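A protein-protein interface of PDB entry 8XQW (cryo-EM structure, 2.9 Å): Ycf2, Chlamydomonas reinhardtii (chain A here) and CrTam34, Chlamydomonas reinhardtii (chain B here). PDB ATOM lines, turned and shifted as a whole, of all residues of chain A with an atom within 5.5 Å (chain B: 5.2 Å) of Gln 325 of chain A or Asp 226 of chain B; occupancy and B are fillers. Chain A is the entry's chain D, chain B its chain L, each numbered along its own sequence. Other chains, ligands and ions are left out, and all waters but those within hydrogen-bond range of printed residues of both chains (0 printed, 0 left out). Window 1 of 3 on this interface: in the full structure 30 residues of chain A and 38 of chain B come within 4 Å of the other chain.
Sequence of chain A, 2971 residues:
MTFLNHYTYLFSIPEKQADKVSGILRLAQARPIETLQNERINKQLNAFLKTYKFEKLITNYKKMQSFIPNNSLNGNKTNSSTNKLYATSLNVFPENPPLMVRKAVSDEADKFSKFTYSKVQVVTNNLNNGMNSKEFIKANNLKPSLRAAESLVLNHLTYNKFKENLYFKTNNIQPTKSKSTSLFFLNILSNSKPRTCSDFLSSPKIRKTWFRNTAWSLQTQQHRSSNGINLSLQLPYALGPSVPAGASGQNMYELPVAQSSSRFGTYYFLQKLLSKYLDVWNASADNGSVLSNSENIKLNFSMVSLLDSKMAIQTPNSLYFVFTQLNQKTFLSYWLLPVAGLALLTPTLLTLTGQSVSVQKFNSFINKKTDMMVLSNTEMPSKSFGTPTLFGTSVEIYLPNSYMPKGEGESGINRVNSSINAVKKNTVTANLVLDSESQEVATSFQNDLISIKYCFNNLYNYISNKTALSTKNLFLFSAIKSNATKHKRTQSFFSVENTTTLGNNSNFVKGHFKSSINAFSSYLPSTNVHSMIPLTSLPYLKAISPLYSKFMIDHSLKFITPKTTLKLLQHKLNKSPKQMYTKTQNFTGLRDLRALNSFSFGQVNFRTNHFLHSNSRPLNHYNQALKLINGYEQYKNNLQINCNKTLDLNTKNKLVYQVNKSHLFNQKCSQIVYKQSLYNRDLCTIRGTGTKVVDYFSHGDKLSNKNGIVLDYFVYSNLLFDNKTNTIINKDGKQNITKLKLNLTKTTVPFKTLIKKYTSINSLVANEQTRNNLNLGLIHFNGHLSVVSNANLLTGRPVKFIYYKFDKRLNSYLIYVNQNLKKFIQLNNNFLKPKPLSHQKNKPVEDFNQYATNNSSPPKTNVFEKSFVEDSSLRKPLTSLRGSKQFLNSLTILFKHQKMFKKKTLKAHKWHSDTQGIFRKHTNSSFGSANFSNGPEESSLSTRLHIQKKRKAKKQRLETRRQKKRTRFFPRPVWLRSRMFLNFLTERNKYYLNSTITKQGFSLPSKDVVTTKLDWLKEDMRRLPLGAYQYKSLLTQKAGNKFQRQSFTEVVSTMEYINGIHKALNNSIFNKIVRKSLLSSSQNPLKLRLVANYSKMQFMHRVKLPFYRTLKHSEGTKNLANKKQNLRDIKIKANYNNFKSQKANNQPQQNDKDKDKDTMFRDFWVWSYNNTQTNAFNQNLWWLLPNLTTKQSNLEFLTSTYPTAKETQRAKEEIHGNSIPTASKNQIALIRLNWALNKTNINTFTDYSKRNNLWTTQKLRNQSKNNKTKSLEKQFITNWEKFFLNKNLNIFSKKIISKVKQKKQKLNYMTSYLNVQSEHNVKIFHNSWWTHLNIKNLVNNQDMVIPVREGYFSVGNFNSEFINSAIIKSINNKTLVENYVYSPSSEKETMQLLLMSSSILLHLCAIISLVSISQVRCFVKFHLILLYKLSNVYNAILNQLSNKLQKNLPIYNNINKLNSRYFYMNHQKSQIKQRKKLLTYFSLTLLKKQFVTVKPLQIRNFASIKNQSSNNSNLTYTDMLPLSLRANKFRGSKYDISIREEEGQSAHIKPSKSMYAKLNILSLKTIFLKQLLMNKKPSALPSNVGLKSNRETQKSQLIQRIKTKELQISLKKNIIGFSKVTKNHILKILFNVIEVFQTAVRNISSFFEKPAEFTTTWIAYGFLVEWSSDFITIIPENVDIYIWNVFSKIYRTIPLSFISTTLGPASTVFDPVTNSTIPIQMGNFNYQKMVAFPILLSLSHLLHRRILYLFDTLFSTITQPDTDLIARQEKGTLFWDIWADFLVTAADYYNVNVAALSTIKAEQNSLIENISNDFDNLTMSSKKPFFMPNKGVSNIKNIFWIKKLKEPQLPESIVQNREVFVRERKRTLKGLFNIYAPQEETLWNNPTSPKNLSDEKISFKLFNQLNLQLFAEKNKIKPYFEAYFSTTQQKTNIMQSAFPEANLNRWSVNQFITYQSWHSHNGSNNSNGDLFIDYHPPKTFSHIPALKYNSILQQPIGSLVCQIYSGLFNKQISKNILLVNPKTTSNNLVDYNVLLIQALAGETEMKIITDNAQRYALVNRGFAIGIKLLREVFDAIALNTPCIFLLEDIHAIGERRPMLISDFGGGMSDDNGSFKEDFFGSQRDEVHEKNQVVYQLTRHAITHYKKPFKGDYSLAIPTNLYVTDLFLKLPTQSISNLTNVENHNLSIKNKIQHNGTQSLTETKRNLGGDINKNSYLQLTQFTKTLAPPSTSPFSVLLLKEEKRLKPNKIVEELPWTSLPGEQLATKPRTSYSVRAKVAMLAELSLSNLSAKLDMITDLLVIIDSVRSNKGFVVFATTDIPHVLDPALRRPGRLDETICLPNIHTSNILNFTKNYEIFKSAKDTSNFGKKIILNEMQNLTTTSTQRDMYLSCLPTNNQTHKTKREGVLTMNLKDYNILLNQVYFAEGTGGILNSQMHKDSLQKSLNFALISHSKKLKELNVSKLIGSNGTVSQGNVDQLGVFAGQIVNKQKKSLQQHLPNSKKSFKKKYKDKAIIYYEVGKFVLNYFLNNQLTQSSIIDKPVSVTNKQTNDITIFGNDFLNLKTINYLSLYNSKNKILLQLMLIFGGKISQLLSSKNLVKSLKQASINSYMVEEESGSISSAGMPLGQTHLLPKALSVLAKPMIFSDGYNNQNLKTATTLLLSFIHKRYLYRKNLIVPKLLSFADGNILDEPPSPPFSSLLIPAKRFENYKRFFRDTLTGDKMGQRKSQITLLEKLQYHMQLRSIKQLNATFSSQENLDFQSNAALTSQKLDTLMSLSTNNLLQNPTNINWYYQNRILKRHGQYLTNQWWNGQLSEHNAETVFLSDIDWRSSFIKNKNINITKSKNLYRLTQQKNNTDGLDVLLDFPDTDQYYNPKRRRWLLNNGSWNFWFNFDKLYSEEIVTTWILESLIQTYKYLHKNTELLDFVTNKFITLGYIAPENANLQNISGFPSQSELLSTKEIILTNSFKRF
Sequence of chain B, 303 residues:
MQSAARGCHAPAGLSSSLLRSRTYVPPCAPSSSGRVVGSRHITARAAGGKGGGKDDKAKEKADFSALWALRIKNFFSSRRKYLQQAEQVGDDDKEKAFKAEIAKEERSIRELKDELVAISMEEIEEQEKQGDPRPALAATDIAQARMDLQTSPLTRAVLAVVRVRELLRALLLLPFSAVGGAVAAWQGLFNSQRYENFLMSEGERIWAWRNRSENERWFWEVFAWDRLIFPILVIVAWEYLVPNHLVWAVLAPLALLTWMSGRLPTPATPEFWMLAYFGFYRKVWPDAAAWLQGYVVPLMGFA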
ATOM      1  N   PHE A 323       1.983  -4.983 -22.388  1.00  0.00           N
ATOM      2  CA  PHE A 323       0.815  -5.795 -22.678  1.00  0.00           C
ATOM      3  C   PHE A 323      -0.455  -5.062 -22.276  1.00  0.00           C
ATOM      4  O   PHE A 323      -0.421  -4.017 -21.631  1.00  0.00           O
ATOM      5  CB  PHE A 323       0.872  -7.114 -21.923  1.00  0.00           C
ATOM      6  CG  PHE A 323       1.896  -8.074 -22.426  1.00  0.00           C
ATOM      7  CD1 PHE A 323       1.629  -8.890 -23.497  1.00  0.00           C
ATOM      8  CD2 PHE A 323       3.108  -8.199 -21.793  1.00  0.00           C
ATOM      9  CE1 PHE A 323       2.552  -9.784 -23.936  1.00  0.00           C
ATOM     10  CE2 PHE A 323       4.038  -9.088 -22.240  1.00  0.00           C
ATOM     11  CZ  PHE A 323       3.756  -9.884 -23.307  1.00  0.00           C
ATOM     12  N   THR A 324      -1.590  -5.635 -22.646  1.00  0.00           N
ATOM     13  CA  THR A 324      -2.880  -5.143 -22.193  1.00  0.00           C
ATOM     14  C   THR A 324      -3.474  -6.136 -21.197  1.00  0.00           C
ATOM     15  O   THR A 324      -2.973  -7.246 -21.025  1.00  0.00           O
ATOM     16  CB  THR A 324      -3.800  -4.887 -23.377  1.00  0.00           C
ATOM     17  OG1 THR A 324      -3.431  -5.750 -24.455  1.00  0.00           O
ATOM     18  CG2 THR A 324      -3.702  -3.457 -23.823  1.00  0.00           C
ATOM     19  N   GLN A 325      -4.565  -5.756 -20.543  1.00  0.00           N
ATOM     20  CA  GLN A 325      -4.953  -6.435 -19.317  1.00  0.00           C
ATOM     21  C   GLN A 325      -5.402  -7.873 -19.534  1.00  0.00           C
ATOM     22  O   GLN A 325      -5.014  -8.752 -18.758  1.00  0.00           O
ATOM     23  CB  GLN A 325      -6.056  -5.657 -18.609  1.00  0.00           C
ATOM     24  CG  GLN A 325      -6.068  -5.899 -17.128  1.00  0.00           C
ATOM     25  CD  GLN A 325      -7.401  -5.608 -16.514  1.00  0.00           C
ATOM     26  OE1 GLN A 325      -7.769  -6.187 -15.498  1.00  0.00           O
ATOM     27  NE2 GLN A 325      -8.144  -4.705 -17.129  1.00  0.00           N
ATOM     28  N   LEU A 326      -6.244  -8.119 -20.536  1.00  0.00           N
ATOM     29  CA  LEU A 326      -6.595  -9.465 -20.988  1.00  0.00           C
ATOM     30  C   LEU A 326      -7.571 -10.202 -20.076  1.00  0.00           C
ATOM     31  O   LEU A 326      -8.037 -11.284 -20.430  1.00  0.00           O
ATOM     32  CB  LEU A 326      -5.329 -10.304 -21.162  1.00  0.00           C
ATOM     33  CG  LEU A 326      -5.385 -11.663 -21.835  1.00  0.00           C
ATOM     34  CD1 LEU A 326      -4.805 -11.528 -23.203  1.00  0.00           C
ATOM     35  CD2 LEU A 326      -4.603 -12.655 -21.032  1.00  0.00           C
ATOM     36  N   ASN A 327      -7.924  -9.645 -18.922  1.00  0.00           N
ATOM     37  CA  ASN A 327      -8.938 -10.318 -18.121  1.00  0.00           C
ATOM     38  C   ASN A 327     -10.036  -9.378 -17.643  1.00  0.00           C
ATOM     39  O   ASN A 327     -10.745  -9.709 -16.688  1.00  0.00           O
ATOM     40  CB  ASN A 327      -8.319 -11.044 -16.919  1.00  0.00           C
ATOM     41  CG  ASN A 327      -7.666 -10.107 -15.920  1.00  0.00           C
ATOM     42  OD1 ASN A 327      -8.099  -8.980 -15.715  1.00  0.00           O
ATOM     43  ND2 ASN A 327      -6.619 -10.595 -15.271  1.00  0.00           N
ATOM     44  N   GLN A 328     -10.198  -8.219 -18.271  1.00  0.00           N
ATOM     45  CA  GLN A 328     -11.272  -7.318 -17.887  1.00  0.00           C
ATOM     46  C   GLN A 328     -12.612  -7.761 -18.438  1.00  0.00           C
ATOM     47  O   GLN A 328     -13.650  -7.319 -17.942  1.00  0.00           O
ATOM     48  CB  GLN A 328     -10.963  -5.900 -18.362  1.00  0.00           C
ATOM     49  CG  GLN A 328     -11.824  -4.820 -17.726  1.00  0.00           C
ATOM     50  CD  GLN A 328     -11.887  -4.927 -16.217  1.00  0.00           C
ATOM     51  OE1 GLN A 328     -10.878  -5.158 -15.556  1.00  0.00           O
ATOM     52  NE2 GLN A 328     -13.078  -4.760 -15.664  1.00  0.00           N
ATOM     53  N   ARG A1746      -3.567 -12.976  -5.195  1.00  0.00           N
ATOM     54  CA  ARG A1746      -4.403 -13.822  -6.036  1.00  0.00           C
ATOM     55  C   ARG A1746      -5.578 -14.379  -5.256  1.00  0.00           C
ATOM     56  O   ARG A1746      -6.687 -14.475  -5.783  1.00  0.00           O
ATOM     57  CB  ARG A1746      -3.583 -14.957  -6.634  1.00  0.00           C
ATOM     58  CG  ARG A1746      -2.977 -14.646  -7.975  1.00  0.00           C
ATOM     59  CD  ARG A1746      -3.864 -13.752  -8.788  1.00  0.00           C
ATOM     60  NE  ARG A1746      -3.435 -12.364  -8.690  1.00  0.00           N
ATOM     61  CZ  ARG A1746      -4.092 -11.346  -9.223  1.00  0.00           C
ATOM     62  NH1 ARG A1746      -5.202 -11.560  -9.905  1.00  0.00           N
ATOM     63  NH2 ARG A1746      -3.633 -10.116  -9.076  1.00  0.00           N
ATOM     64  N   LEU A1944     -12.431  -0.120 -19.359  1.00  0.00           N
ATOM     65  CA  LEU A1944     -10.993   0.030 -19.176  1.00  0.00           C
ATOM     66  C   LEU A1944     -10.590  -0.134 -17.715  1.00  0.00           C
ATOM     67  O   LEU A1944      -9.422   0.026 -17.366  1.00  0.00           O
ATOM     68  CB  LEU A1944     -10.528   1.390 -19.704  1.00  0.00           C
ATOM     69  CG  LEU A1944      -9.049   1.545 -20.075  1.00  0.00           C
ATOM     70  CD1 LEU A1944      -8.417   0.207 -20.424  1.00  0.00           C
ATOM     71  CD2 LEU A1944      -8.892   2.519 -21.227  1.00  0.00           C
ATOM     72  N   ASN A1945     -11.557  -0.478 -16.865  1.00  0.00           N
ATOM     73  CA  ASN A1945     -11.315  -0.641 -15.436  1.00  0.00           C
ATOM     74  C   ASN A1945     -10.765   0.655 -14.836  1.00  0.00           C
ATOM     75  O   ASN A1945      -9.589   0.781 -14.503  1.00  0.00           O
ATOM     76  CB  ASN A1945     -10.377  -1.815 -15.150  1.00  0.00           C
ATOM     77  CG  ASN A1945     -10.442  -2.261 -13.709  1.00  0.00           C
ATOM     78  OD1 ASN A1945     -11.389  -1.943 -12.996  1.00  0.00           O
ATOM     79  ND2 ASN A1945      -9.434  -3.001 -13.271  1.00  0.00           N
ATOM     80  N   SER A1948      -8.260   1.205 -11.957  1.00  0.00           N
ATOM     81  CA  SER A1948      -6.832   0.956 -12.012  1.00  0.00           C
ATOM     82  C   SER A1948      -6.007   2.216 -11.875  1.00  0.00           C
ATOM     83  O   SER A1948      -4.839   2.130 -11.499  1.00  0.00           O
ATOM     84  CB  SER A1948      -6.460   0.270 -13.320  1.00  0.00           C
ATOM     85  OG  SER A1948      -7.228  -0.898 -13.501  1.00  0.00           O
ATOM     86  N   GLU B 221       0.520  -3.589  -7.250  1.00  0.00           N
ATOM     87  CA  GLU B 221      -0.912  -3.786  -7.080  1.00  0.00           C
ATOM     88  C   GLU B 221      -1.675  -3.905  -8.385  1.00  0.00           C
ATOM     89  O   GLU B 221      -2.689  -4.600  -8.425  1.00  0.00           O
ATOM     90  CB  GLU B 221      -1.518  -2.645  -6.275  1.00  0.00           C
ATOM     91  CG  GLU B 221      -1.039  -2.567  -4.858  1.00  0.00           C
ATOM     92  CD  GLU B 221      -1.789  -3.496  -3.947  1.00  0.00           C
ATOM     93  OE1 GLU B 221      -2.959  -3.796  -4.247  1.00  0.00           O
ATOM     94  OE2 GLU B 221      -1.210  -3.929  -2.932  1.00  0.00           O
ATOM     95  N   VAL B 222      -1.238  -3.248  -9.452  1.00  0.00           N
ATOM     96  CA  VAL B 222      -2.070  -3.136 -10.642  1.00  0.00           C
ATOM     97  C   VAL B 222      -1.373  -3.685 -11.877  1.00  0.00           C
ATOM     98  O   VAL B 222      -2.023  -4.045 -12.859  1.00  0.00           O
ATOM     99  CB  VAL B 222      -2.489  -1.675 -10.847  1.00  0.00           C
ATOM    100  CG1 VAL B 222      -3.313  -1.527 -12.073  1.00  0.00           C
ATOM    101  CG2 VAL B 222      -3.281  -1.204  -9.671  1.00  0.00           C
ATOM    102  N   PHE B 223      -0.059  -3.792 -11.843  1.00  0.00           N
ATOM    103  CA  PHE B 223       0.678  -4.092 -13.056  1.00  0.00           C
ATOM    104  C   PHE B 223       1.405  -5.422 -13.041  1.00  0.00           C
ATOM    105  O   PHE B 223       1.592  -6.008 -14.094  1.00  0.00           O
ATOM    106  CB  PHE B 223       1.686  -2.985 -13.324  1.00  0.00           C
ATOM    107  CG  PHE B 223       2.273  -3.023 -14.684  1.00  0.00           C
ATOM    108  CD1 PHE B 223       1.631  -2.431 -15.731  1.00  0.00           C
ATOM    109  CD2 PHE B 223       3.477  -3.627 -14.909  1.00  0.00           C
ATOM    110  CE1 PHE B 223       2.171  -2.466 -16.972  1.00  0.00           C
ATOM    111  CE2 PHE B 223       4.012  -3.658 -16.150  1.00  0.00           C
ATOM    112  CZ  PHE B 223       3.364  -3.076 -17.179  1.00  0.00           C
ATOM    113  N   ALA B 224       1.834  -5.926 -11.889  1.00  0.00           N
ATOM    114  CA  ALA B 224       2.726  -7.077 -11.904  1.00  0.00           C
ATOM    115  C   ALA B 224       2.056  -8.291 -12.519  1.00  0.00           C
ATOM    116  O   ALA B 224       2.544  -8.840 -13.505  1.00  0.00           O
ATOM    117  CB  ALA B 224       3.203  -7.397 -10.497  1.00  0.00           C
ATOM    118  N   TRP B 225       0.939  -8.730 -11.953  1.00  0.00           N
ATOM    119  CA  TRP B 225       0.275  -9.915 -12.473  1.00  0.00           C
ATOM    120  C   TRP B 225      -0.491  -9.609 -13.746  1.00  0.00           C
ATOM    121  O   TRP B 225      -0.265 -10.229 -14.783  1.00  0.00           O
ATOM    122  CB  TRP B 225      -0.662 -10.487 -11.420  1.00  0.00           C
ATOM    123  CG  TRP B 225      -1.404 -11.693 -11.864  1.00  0.00           C
ATOM    124  CD1 TRP B 225      -2.662 -11.740 -12.347  1.00  0.00           C
ATOM    125  CD2 TRP B 225      -0.932 -13.034 -11.843  1.00  0.00           C
ATOM    126  NE1 TRP B 225      -3.005 -13.023 -12.644  1.00  0.00           N
ATOM    127  CE2 TRP B 225      -1.955 -13.840 -12.338  1.00  0.00           C
ATOM    128  CE3 TRP B 225       0.266 -13.629 -11.462  1.00  0.00           C
ATOM    129  CZ2 TRP B 225      -1.822 -15.206 -12.461  1.00  0.00           C
ATOM    130  CZ3 TRP B 225       0.393 -14.977 -11.585  1.00  0.00           C
ATOM    131  CH2 TRP B 225      -0.640 -15.755 -12.079  1.00  0.00           C
ATOM    132  N   ASP B 226      -1.382  -8.630 -13.689  1.00  0.00           N
ATOM    133  CA  ASP B 226      -2.388  -8.473 -14.727  1.00  0.00           C
ATOM    134  C   ASP B 226      -1.798  -8.129 -16.082  1.00  0.00           C
ATOM    135  O   ASP B 226      -2.355  -8.531 -17.104  1.00  0.00           O
ATOM    136  CB  ASP B 226      -3.379  -7.412 -14.297  1.00  0.00           C
ATOM    137  CG  ASP B 226      -3.928  -7.675 -12.918  1.00  0.00           C
ATOM    138  OD1 ASP B 226      -4.821  -8.536 -12.793  1.00  0.00           O
ATOM    139  OD2 ASP B 226      -3.467  -7.036 -11.952  1.00  0.00           O
ATOM    140  N   ARG B 227      -0.692  -7.399 -16.128  1.00  0.00           N
ATOM    141  CA  ARG B 227      -0.148  -6.950 -17.395  1.00  0.00           C
ATOM    142  C   ARG B 227       1.283  -7.379 -17.644  1.00  0.00           C
ATOM    143  O   ARG B 227       1.870  -6.939 -18.630  1.00  0.00           O
ATOM    144  CB  ARG B 227      -0.225  -5.428 -17.501  1.00  0.00           C
ATOM    145  CG  ARG B 227      -1.616  -4.897 -17.408  1.00  0.00           C
ATOM    146  CD  ARG B 227      -1.642  -3.410 -17.523  1.00  0.00           C
ATOM    147  NE  ARG B 227      -1.176  -2.972 -18.827  1.00  0.00           N
ATOM    148  CZ  ARG B 227      -1.268  -1.725 -19.265  1.00  0.00           C
ATOM    149  NH1 ARG B 227      -1.800  -0.795 -18.504  1.00  0.00           N
ATOM    150  NH2 ARG B 227      -0.821  -1.407 -20.458  1.00  0.00           N
ATOM    151  N   LEU B 228       1.885  -8.182 -16.780  1.00  0.00           N
ATOM    152  CA  LEU B 228       3.231  -8.668 -17.046  1.00  0.00           C
ATOM    153  C   LEU B 228       3.327 -10.185 -17.010  1.00  0.00           C
ATOM    154  O   LEU B 228       3.892 -10.774 -17.930  1.00  0.00           O
ATOM    155  CB  LEU B 228       4.212  -8.040 -16.059  1.00  0.00           C
ATOM    156  CG  LEU B 228       5.682  -8.373 -16.252  1.00  0.00           C
ATOM    157  CD1 LEU B 228       6.130  -7.956 -17.612  1.00  0.00           C
ATOM    158  CD2 LEU B 228       6.478  -7.660 -15.210  1.00  0.00           C
ATOM    159  N   PHE B 230       0.662 -12.612 -16.248  1.00  0.00           N
ATOM    160  CA  PHE B 230      -0.464 -13.366 -16.774  1.00  0.00           C
ATOM    161  C   PHE B 230      -0.436 -13.523 -18.285  1.00  0.00           C
ATOM    162  O   PHE B 230      -0.649 -14.650 -18.752  1.00  0.00           O
ATOM    163  CB  PHE B 230      -1.774 -12.728 -16.325  1.00  0.00           C
ATOM    164  CG  PHE B 230      -2.961 -13.588 -16.559  1.00  0.00           C
ATOM    165  CD1 PHE B 230      -2.996 -14.870 -16.072  1.00  0.00           C
ATOM    166  CD2 PHE B 230      -4.034 -13.125 -17.272  1.00  0.00           C
ATOM    167  CE1 PHE B 230      -4.074 -15.663 -16.286  1.00  0.00           C
ATOM    168  CE2 PHE B 230      -5.111 -13.920 -17.490  1.00  0.00           C
ATOM    169  CZ  PHE B 230      -5.131 -15.190 -16.995  1.00  0.00           C
ATOM    170  N   PRO B 231      -0.200 -12.489 -19.096  1.00  0.00           N
ATOM    171  CA  PRO B 231      -0.205 -12.720 -20.543  1.00  0.00           C
ATOM    172  C   PRO B 231       0.936 -13.593 -21.019  1.00  0.00           C
ATOM    173  O   PRO B 231       0.758 -14.398 -21.940  1.00  0.00           O
ATOM    174  CB  PRO B 231      -0.117 -11.303 -21.106  1.00  0.00           C
ATOM    175  CG  PRO B 231      -0.670 -10.474 -20.060  1.00  0.00           C
ATOM    176  CD  PRO B 231      -0.139 -11.051 -18.818  1.00  0.00           C
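O of Asp 226 of chain B sits close to O of Gln 325 of chain A (3.1 Å).
NH2 of Arg 227 of chain B is in hydrogen-bond range of O of Phe 323 of chain A.
OE1 of Gln 328 of chain A sits at hydrogen-bond distance from NE2 of Gln 325 of chain A (3.2 Å).
The side-chain amide nitrogen of Asn 1945 of chain A sits at hydrogen-bond distance from the side-chain hydroxyl of Ser 1948 of chain A, at 3.1 Å.
The backbone carbonyl oxygen (O) of Trp 225 of chain B sits at hydrogen-bond distance from the backbone NH (N) of Phe 230 of chain B, 2.9 Å away.
OE1 of Gln 325 of chain A sits close to OD1 of Asn 327 of chain A (2.8 Å).
Among the printed residues, pairs that only touch across the chains: Arg 1746 of chain A with Trp 225 of chain B (3.5 Å), Asn 327 of chain A with Asp 226 of chain B (3.7 Å), Leu 326 of chain A with Phe 230 of chain B (3.8 Å), Phe 323 of chain A with Pro 231 of chain B (3.8 Å) and Ser 1948 of chain A with Val 222 of chain B (3.8 Å).
Of the printed residues of chain B, Phe 323 of chain A touches Arg 227 (2.9 Å) and Pro 231 (3.8 Å).
Thr 324 of chain A touches none of the printed residues of chain B.
Gln 325 of chain A touches one residue of chain B.
Of the printed residues of chain B, Arg 1746 of chain A touches Trp 225 (3.5 Å).
Leu 1944 of chain A touches none of the printed residues of chain B.
Of the printed residues of chain B, Ser 1948 of chain A touches Val 222 (3.8 Å).
Of the printed residues of chain A, Val 222 of chain B touches Ser 1948.
Asp 226 of chain B touches two residues of chain A.
Of the printed residues of chain A, Pro 231 of chain B touches Phe 323.
The nearest residue of chain B that does not touch Gln 325 of chain A is Arg 227 of chain B (4.1 Å).
The nearest printed residue of chain A that does not touch Asp 226 of chain B is Thr 324 of chain A (4.2 Å).
The nearest printed residue of chain B that does not touch Ser 1948 of chain A is Arg 227 of chain B (7.1 Å).
Hydrophobic or aromatic side chains of chain A that line the printed part of chain B: Phe 323 and Leu 326.
Among the printed residues, 7 pairs touch across the chains.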
